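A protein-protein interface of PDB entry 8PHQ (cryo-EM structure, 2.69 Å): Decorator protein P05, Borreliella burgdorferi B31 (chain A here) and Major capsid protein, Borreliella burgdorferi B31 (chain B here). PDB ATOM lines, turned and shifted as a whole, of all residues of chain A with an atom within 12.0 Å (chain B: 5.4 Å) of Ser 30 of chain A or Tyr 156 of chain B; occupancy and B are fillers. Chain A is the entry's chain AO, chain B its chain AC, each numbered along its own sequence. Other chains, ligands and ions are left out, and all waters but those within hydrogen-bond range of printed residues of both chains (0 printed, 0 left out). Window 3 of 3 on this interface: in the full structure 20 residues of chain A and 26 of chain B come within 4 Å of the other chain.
The backbone carbonyl oxygen (O) of Arg 78 of chain B sits at hydrogen-bond distance from the side-chain amide nitrogen (ND2) of Asn 154 of chain B (3.0 Å).
Printed residues of chain A that touch a printed residue of chain B: Ala 29, Ser 30, Leu 31 and Leu 32.
Hydrophobic or aromatic side chains of chain A within 4 Å of the printed part of chain B: Leu 31 and Leu 32.
Among the printed residues, no Asp or Glu carboxylate lies within 4 Å of a Lys or Arg side-chain nitrogen of the other chain.
Ser 30 of chain A touches just these residues of chain B: Val 77, Asn 154, Tyr 156 and Pro 162.
Val 77 of chain B touches just these residues of chain A: Ala 29 (3.3 Å), Ser 30 (3.8 Å), Leu 31 (3.7 Å) and Leu 32 (3.7 Å).
Gly 137 of chain B touches none of the printed residues of chain A.
Pro 153 of chain B touches none of the printed residues of chain A.
No residue of chain A comes within 4 Å of Met 155 of chain B.
No residue of chain A comes within 4 Å of Asn 160 of chain B.
Pro 162 of chain B touches just these residues of chain A: Ser 30 and Leu 31.
No residue of chain A comes within 4 Å of Leu 304 of chain B.
Of the printed residues of chain B, Leu 32 of chain A touches Val 77.
Printed residues of chain B within 4 Å of Leu 31 of chain A: Val 77 and Pro 162.
Leu 158 of chain B touches none of the printed residues of chain A.
Asp 28 of chain A touches none of the printed residues of chain B.
The nearest residue of chain A that does not touch Tyr 156 of chain B is Leu 31 of chain A (6.2 Å).
The nearest printed residue of chain B that does not touch Ala 29 of chain A is Leu 79 of chain B (6.1 Å).
The backbone carbonyl oxygen of Ala 29 of chain A sits at hydrogen-bond distance from the backbone NH of Arg 78 of chain B (3.3 Å).
Among the printed residues, pairs that only touch across the chains: Ser 30 of chain A with Asn 154 of chain B, Leu 31 of chain A with Pro 162 of chain B, Ala 29 of chain A with Val 77 of chain B, Ser 30 of chain A with Tyr 156 of chain B, Ala 29 of chain A with Asn 154 of chain B, Leu 31 of chain A with Val 77 of chain B, Leu 32 of chain A with Val 77 of chain B, Ser 30 of chain A with Val 77 of chain B and Ser 30 of chain A with Pro 162 of chain B.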
ATOM      1  N   ASN A  24       3.909 -25.408   9.676  1.00  0.00           N
ATOM      2  CA  ASN A  24       5.319 -25.697   9.927  1.00  0.00           C
ATOM      3  C   ASN A  24       6.055 -24.384  10.150  1.00  0.00           C
ATOM      4  O   ASN A  24       6.521 -23.750   9.190  1.00  0.00           O
ATOM      5  CB  ASN A  24       5.938 -26.472   8.767  1.00  0.00           C
ATOM      6  CG  ASN A  24       5.381 -27.872   8.632  1.00  0.00           C
ATOM      7  OD1 ASN A  24       4.507 -28.284   9.394  1.00  0.00           O
ATOM      8  ND2 ASN A  24       5.889 -28.616   7.658  1.00  0.00           N
ATOM      9  N   PRO A  25       6.188 -23.936  11.397  1.00  0.00           N
ATOM     10  CA  PRO A  25       6.947 -22.712  11.684  1.00  0.00           C
ATOM     11  C   PRO A  25       8.444 -22.914  11.861  1.00  0.00           C
ATOM     12  O   PRO A  25       9.132 -21.959  12.233  1.00  0.00           O
ATOM     13  CB  PRO A  25       6.310 -22.247  12.998  1.00  0.00           C
ATOM     14  CG  PRO A  25       5.999 -23.529  13.704  1.00  0.00           C
ATOM     15  CD  PRO A  25       5.673 -24.556  12.630  1.00  0.00           C
ATOM     16  N   GLN A  26       8.962 -24.113  11.610  1.00  0.00           N
ATOM     17  CA  GLN A  26      10.381 -24.400  11.761  1.00  0.00           C
ATOM     18  C   GLN A  26      11.164 -24.241  10.465  1.00  0.00           C
ATOM     19  O   GLN A  26      12.377 -24.470  10.462  1.00  0.00           O
ATOM     20  CB  GLN A  26      10.578 -25.817  12.304  1.00  0.00           C
ATOM     21  CG  GLN A  26       9.840 -26.089  13.602  1.00  0.00           C
ATOM     22  CD  GLN A  26      10.196 -25.098  14.692  1.00  0.00           C
ATOM     23  OE1 GLN A  26       9.335 -24.379  15.199  1.00  0.00           O
ATOM     24  NE2 GLN A  26      11.472 -25.058  15.062  1.00  0.00           N
ATOM     25  N   HIS A  27      10.510 -23.858   9.370  1.00  0.00           N
ATOM     26  CA  HIS A  27      11.220 -23.632   8.118  1.00  0.00           C
ATOM     27  C   HIS A  27      11.821 -22.237   8.029  1.00  0.00           C
ATOM     28  O   HIS A  27      12.491 -21.930   7.038  1.00  0.00           O
ATOM     29  CB  HIS A  27      10.292 -23.875   6.926  1.00  0.00           C
ATOM     30  CG  HIS A  27       9.706 -25.250   6.893  1.00  0.00           C
ATOM     31  ND1 HIS A  27      10.452 -26.382   7.137  1.00  0.00           N
ATOM     32  CD2 HIS A  27       8.450 -25.678   6.625  1.00  0.00           C
ATOM     33  CE1 HIS A  27       9.679 -27.448   7.038  1.00  0.00           C
ATOM     34  NE2 HIS A  27       8.459 -27.049   6.724  1.00  0.00           N
ATOM     35  N   ASP A  28      11.597 -21.393   9.033  1.00  0.00           N
ATOM     36  CA  ASP A  28      12.248 -20.096   9.141  1.00  0.00           C
ATOM     37  C   ASP A  28      13.218 -20.066  10.319  1.00  0.00           C
ATOM     38  O   ASP A  28      13.435 -19.019  10.932  1.00  0.00           O
ATOM     39  CB  ASP A  28      11.209 -18.983   9.267  1.00  0.00           C
ATOM     40  CG  ASP A  28      11.755 -17.628   8.866  1.00  0.00           C
ATOM     41  OD1 ASP A  28      12.192 -17.482   7.705  1.00  0.00           O
ATOM     42  OD2 ASP A  28      11.746 -16.708   9.711  1.00  0.00           O
ATOM     43  N   ALA A  29      13.795 -21.219  10.648  1.00  0.00           N
ATOM     44  CA  ALA A  29      14.695 -21.316  11.786  1.00  0.00           C
ATOM     45  C   ALA A  29      15.966 -20.516  11.536  1.00  0.00           C
ATOM     46  O   ALA A  29      16.509 -20.507  10.428  1.00  0.00           O
ATOM     47  CB  ALA A  29      15.042 -22.776  12.067  1.00  0.00           C
ATOM     48  N   SER A  30      16.435 -19.834  12.578  1.00  0.00           N
ATOM     49  CA  SER A  30      17.651 -19.041  12.487  1.00  0.00           C
ATOM     50  C   SER A  30      18.908 -19.835  12.809  1.00  0.00           C
ATOM     51  O   SER A  30      20.010 -19.378  12.487  1.00  0.00           O
ATOM     52  CB  SER A  30      17.560 -17.836  13.425  1.00  0.00           C
ATOM     53  OG  SER A  30      17.271 -18.243  14.750  1.00  0.00           O
ATOM     54  N   LEU A  31      18.773 -21.005  13.429  1.00  0.00           N
ATOM     55  CA  LEU A  31      19.930 -21.796  13.818  1.00  0.00           C
ATOM     56  C   LEU A  31      19.537 -23.265  13.881  1.00  0.00           C
ATOM     57  O   LEU A  31      18.359 -23.610  13.998  1.00  0.00           O
ATOM     58  CB  LEU A  31      20.505 -21.335  15.164  1.00  0.00           C
ATOM     59  CG  LEU A  31      19.741 -21.659  16.451  1.00  0.00           C
ATOM     60  CD1 LEU A  31      20.650 -21.460  17.652  1.00  0.00           C
ATOM     61  CD2 LEU A  31      18.485 -20.813  16.597  1.00  0.00           C
ATOM     62  N   LEU A  32      20.547 -24.128  13.797  1.00  0.00           N
ATOM     63  CA  LEU A  32      20.321 -25.564  13.875  1.00  0.00           C
ATOM     64  C   LEU A  32      19.860 -25.960  15.273  1.00  0.00           C
ATOM     65  O   LEU A  32      20.326 -25.415  16.276  1.00  0.00           O
ATOM     66  CB  LEU A  32      21.597 -26.322  13.515  1.00  0.00           C
ATOM     67  CG  LEU A  32      22.033 -26.288  12.050  1.00  0.00           C
ATOM     68  CD1 LEU A  32      23.341 -27.037  11.869  1.00  0.00           C
ATOM     69  CD2 LEU A  32      20.953 -26.877  11.162  1.00  0.00           C
ATOM     70  N   SER A  33      18.942 -26.917  15.333  1.00  0.00           N
ATOM     71  CA  SER A  33      18.460 -27.431  16.605  1.00  0.00           C
ATOM     72  C   SER A  33      19.380 -28.536  17.114  1.00  0.00           C
ATOM     73  O   SER A  33      20.123 -29.161  16.355  1.00  0.00           O
ATOM     74  CB  SER A  33      17.031 -27.956  16.472  1.00  0.00           C
ATOM     75  OG  SER A  33      16.979 -29.084  15.619  1.00  0.00           O
ATOM     76  N   ASN A  34      19.319 -28.770  18.421  1.00  0.00           N
ATOM     77  CA  ASN A  34      20.123 -29.794  19.075  1.00  0.00           C
ATOM     78  C   ASN A  34      19.243 -31.012  19.329  1.00  0.00           C
ATOM     79  O   ASN A  34      18.188 -30.898  19.960  1.00  0.00           O
ATOM     80  CB  ASN A  34      20.716 -29.267  20.380  1.00  0.00           C
ATOM     81  CG  ASN A  34      21.949 -30.033  20.810  1.00  0.00           C
ATOM     82  OD1 ASN A  34      22.373 -30.973  20.138  1.00  0.00           O
ATOM     83  ND2 ASN A  34      22.536 -29.630  21.929  1.00  0.00           N
ATOM     84  N   VAL B  77      16.899 -24.009   7.953  1.00  0.00           N
ATOM     85  CA  VAL B  77      17.678 -22.909   8.502  1.00  0.00           C
ATOM     86  C   VAL B  77      18.157 -22.048   7.347  1.00  0.00           C
ATOM     87  O   VAL B  77      18.756 -22.554   6.388  1.00  0.00           O
ATOM     88  CB  VAL B  77      18.861 -23.422   9.338  1.00  0.00           C
ATOM     89  CG1 VAL B  77      19.603 -22.255   9.958  1.00  0.00           C
ATOM     90  CG2 VAL B  77      18.370 -24.375  10.411  1.00  0.00           C
ATOM     91  N   ARG B  78      17.884 -20.750   7.432  1.00  0.00           N
ATOM     92  CA  ARG B  78      18.160 -19.804   6.363  1.00  0.00           C
ATOM     93  C   ARG B  78      19.202 -18.802   6.834  1.00  0.00           C
ATOM     94  O   ARG B  78      19.093 -18.257   7.937  1.00  0.00           O
ATOM     95  CB  ARG B  78      16.873 -19.095   5.938  1.00  0.00           C
ATOM     96  CG  ARG B  78      17.048 -18.010   4.901  1.00  0.00           C
ATOM     97  CD  ARG B  78      15.698 -17.582   4.358  1.00  0.00           C
ATOM     98  NE  ARG B  78      15.740 -16.260   3.747  1.00  0.00           N
ATOM     99  CZ  ARG B  78      14.708 -15.684   3.147  1.00  0.00           C
ATOM    100  NH1 ARG B  78      13.541 -16.298   3.038  1.00  0.00           N
ATOM    101  NH2 ARG B  78      14.849 -14.461   2.645  1.00  0.00           N
ATOM    102  N   LEU B  79      20.215 -18.574   6.005  1.00  0.00           N
ATOM    103  CA  LEU B  79      21.269 -17.605   6.275  1.00  0.00           C
ATOM    104  C   LEU B  79      21.171 -16.491   5.243  1.00  0.00           C
ATOM    105  O   LEU B  79      21.200 -16.759   4.038  1.00  0.00           O
ATOM    106  CB  LEU B  79      22.647 -18.265   6.224  1.00  0.00           C
ATOM    107  CG  LEU B  79      23.050 -19.129   7.419  1.00  0.00           C
ATOM    108  CD1 LEU B  79      24.507 -19.538   7.311  1.00  0.00           C
ATOM    109  CD2 LEU B  79      22.798 -18.388   8.720  1.00  0.00           C
ATOM    110  N   PHE B 133      30.755  -6.501  13.927  1.00  0.00           N
ATOM    111  CA  PHE B 133      29.539  -7.237  13.589  1.00  0.00           C
ATOM    112  C   PHE B 133      29.690  -8.721  13.885  1.00  0.00           C
ATOM    113  O   PHE B 133      28.816  -9.330  14.511  1.00  0.00           O
ATOM    114  CB  PHE B 133      29.170  -7.051  12.120  1.00  0.00           C
ATOM    115  CG  PHE B 133      28.069  -7.970  11.669  1.00  0.00           C
ATOM    116  CD1 PHE B 133      26.794  -7.855  12.194  1.00  0.00           C
ATOM    117  CD2 PHE B 133      28.324  -8.983  10.762  1.00  0.00           C
ATOM    118  CE1 PHE B 133      25.788  -8.711  11.796  1.00  0.00           C
ATOM    119  CE2 PHE B 133      27.321  -9.842  10.363  1.00  0.00           C
ATOM    120  CZ  PHE B 133      26.052  -9.705  10.880  1.00  0.00           C
ATOM    121  N   GLY B 137      27.117  -9.055  16.420  1.00  0.00           N
ATOM    122  CA  GLY B 137      25.900  -9.189  15.648  1.00  0.00           C
ATOM    123  C   GLY B 137      25.103  -7.919  15.461  1.00  0.00           C
ATOM    124  O   GLY B 137      23.938  -7.995  15.056  1.00  0.00           O
ATOM    125  N   PRO B 153      16.463 -10.590   9.159  1.00  0.00           N
ATOM    126  CA  PRO B 153      16.407 -11.700  10.113  1.00  0.00           C
ATOM    127  C   PRO B 153      17.406 -12.783   9.743  1.00  0.00           C
ATOM    128  O   PRO B 153      17.894 -12.860   8.613  1.00  0.00           O
ATOM    129  CB  PRO B 153      14.964 -12.207   9.992  1.00  0.00           C
ATOM    130  CG  PRO B 153      14.210 -11.066   9.395  1.00  0.00           C
ATOM    131  CD  PRO B 153      15.176 -10.394   8.474  1.00  0.00           C
ATOM    132  N   ASN B 154      17.718 -13.620  10.733  1.00  0.00           N
ATOM    133  CA  ASN B 154      18.697 -14.697  10.581  1.00  0.00           C
ATOM    134  C   ASN B 154      20.081 -14.143  10.249  1.00  0.00           C
ATOM    135  O   ASN B 154      20.818 -14.704   9.438  1.00  0.00           O
ATOM    136  CB  ASN B 154      18.252 -15.712   9.526  1.00  0.00           C
ATOM    137  CG  ASN B 154      16.948 -16.392   9.885  1.00  0.00           C
ATOM    138  OD1 ASN B 154      16.375 -16.141  10.944  1.00  0.00           O
ATOM    139  ND2 ASN B 154      16.472 -17.260   9.001  1.00  0.00           N
ATOM    140  N   MET B 155      20.432 -13.026  10.882  1.00  0.00           N
ATOM    141  CA  MET B 155      21.757 -12.421  10.767  1.00  0.00           C
ATOM    142  C   MET B 155      22.235 -12.133  12.187  1.00  0.00           C
ATOM    143  O   MET B 155      21.844 -11.127  12.786  1.00  0.00           O
ATOM    144  CB  MET B 155      21.720 -11.154   9.921  1.00  0.00           C
ATOM    145  CG  MET B 155      21.824 -11.406   8.427  1.00  0.00           C
ATOM    146  SD  MET B 155      21.740  -9.893   7.456  1.00  0.00           S
ATOM    147  CE  MET B 155      23.426  -9.313   7.601  1.00  0.00           C
ATOM    148  N   TYR B 156      23.075 -13.014  12.724  1.00  0.00           N
ATOM    149  CA  TYR B 156      23.454 -12.968  14.127  1.00  0.00           C
ATOM    150  C   TYR B 156      24.965 -13.058  14.274  1.00  0.00           C
ATOM    151  O   TYR B 156      25.682 -13.468  13.357  1.00  0.00           O
ATOM    152  CB  TYR B 156      22.795 -14.103  14.919  1.00  0.00           C
ATOM    153  CG  TYR B 156      21.290 -14.016  14.977  1.00  0.00           C
ATOM    154  CD1 TYR B 156      20.661 -13.011  15.697  1.00  0.00           C
ATOM    155  CD2 TYR B 156      20.497 -14.934  14.306  1.00  0.00           C
ATOM    156  CE1 TYR B 156      19.288 -12.927  15.752  1.00  0.00           C
ATOM    157  CE2 TYR B 156      19.123 -14.856  14.354  1.00  0.00           C
ATOM    158  CZ  TYR B 156      18.524 -13.852  15.078  1.00  0.00           C
ATOM    159  OH  TYR B 156      17.152 -13.772  15.127  1.00  0.00           O
ATOM    160  N   GLY B 157      25.440 -12.661  15.455  1.00  0.00           N
ATOM    161  CA  GLY B 157      26.824 -12.805  15.834  1.00  0.00           C
ATOM    162  C   GLY B 157      26.991 -13.786  16.985  1.00  0.00           C
ATOM    163  O   GLY B 157      26.040 -14.383  17.482  1.00  0.00           O
ATOM    164  N   LEU B 158      28.249 -13.942  17.402  1.00  0.00           N
ATOM    165  CA  LEU B 158      28.556 -14.875  18.482  1.00  0.00           C
ATOM    166  C   LEU B 158      27.911 -14.458  19.795  1.00  0.00           C
ATOM    167  O   LEU B 158      27.642 -15.309  20.650  1.00  0.00           O
ATOM    168  CB  LEU B 158      30.069 -14.999  18.660  1.00  0.00           C
ATOM    169  CG  LEU B 158      30.837 -15.708  17.545  1.00  0.00           C
ATOM    170  CD1 LEU B 158      32.333 -15.565  17.758  1.00  0.00           C
ATOM    171  CD2 LEU B 158      30.443 -17.169  17.485  1.00  0.00           C
ATOM    172  N   ASN B 160      24.969 -12.416  20.201  1.00  0.00           N
ATOM    173  CA  ASN B 160      23.516 -12.288  20.199  1.00  0.00           C
ATOM    174  C   ASN B 160      22.815 -13.482  19.563  1.00  0.00           C
ATOM    175  O   ASN B 160      21.622 -13.393  19.254  1.00  0.00           O
ATOM    176  CB  ASN B 160      23.091 -10.989  19.503  1.00  0.00           C
ATOM    177  CG  ASN B 160      23.335 -11.010  18.003  1.00  0.00           C
ATOM    178  OD1 ASN B 160      23.960 -11.924  17.467  1.00  0.00           O
ATOM    179  ND2 ASN B 160      22.825  -9.996  17.317  1.00  0.00           N
ATOM    180  N   MET B 161      23.520 -14.589  19.359  1.00  0.00           N
ATOM    181  CA  MET B 161      22.893 -15.780  18.808  1.00  0.00           C
ATOM    182  C   MET B 161      21.831 -16.292  19.776  1.00  0.00           C
ATOM    183  O   MET B 161      22.129 -16.503  20.959  1.00  0.00           O
ATOM    184  CB  MET B 161      23.942 -16.859  18.553  1.00  0.00           C
ATOM    185  CG  MET B 161      23.417 -18.102  17.862  1.00  0.00           C
ATOM    186  SD  MET B 161      22.857 -17.783  16.181  1.00  0.00           S
ATOM    187  CE  MET B 161      24.422 -17.719  15.317  1.00  0.00           C
ATOM    188  N   PRO B 162      20.598 -16.499  19.328  1.00  0.00           N
ATOM    189  CA  PRO B 162      19.534 -16.927  20.238  1.00  0.00           C
ATOM    190  C   PRO B 162      19.652 -18.404  20.592  1.00  0.00           C
ATOM    191  O   PRO B 162      20.395 -19.169  19.976  1.00  0.00           O
ATOM    192  CB  PRO B 162      18.263 -16.645  19.434  1.00  0.00           C
ATOM    193  CG  PRO B 162      18.690 -16.857  18.027  1.00  0.00           C
ATOM    194  CD  PRO B 162      20.100 -16.322  17.952  1.00  0.00           C
ATOM    195  N   LEU B 304      26.675 -16.573   9.803  1.00  0.00           N
ATOM    196  CA  LEU B 304      27.059 -17.310  11.002  1.00  0.00           C
ATOM    197  C   LEU B 304      25.995 -18.356  11.306  1.00  0.00           C
ATOM    198  O   LEU B 304      24.810 -18.024  11.411  1.00  0.00           O
ATOM    199  CB  LEU B 304      27.246 -16.371  12.193  1.00  0.00           C
ATOM    200  CG  LEU B 304      27.902 -17.023  13.410  1.00  0.00           C
ATOM    201  CD1 LEU B 304      29.255 -17.605  13.035  1.00  0.00           C
ATOM    202  CD2 LEU B 304      28.043 -16.024  14.539  1.00  0.00           C
ATOM    203  N   LEU B 305      26.411 -19.615  11.449  1.00  0.00           N
ATOM    204  CA  LEU B 305      25.507 -20.719  11.735  1.00  0.00           C
ATOM    205  C   LEU B 305      25.986 -21.431  12.990  1.00  0.00           C
ATOM    206  O   LEU B 305      27.172 -21.747  13.111  1.00  0.00           O
ATOM    207  CB  LEU B 305      25.450 -21.690  10.553  1.00  0.00           C
ATOM    208  CG  LEU B 305      24.556 -22.919  10.704  1.00  0.00           C
ATOM    209  CD1 LEU B 305      23.106 -22.499  10.795  1.00  0.00           C
ATOM    210  CD2 LEU B 305      24.767 -23.874   9.543  1.00  0.00           C
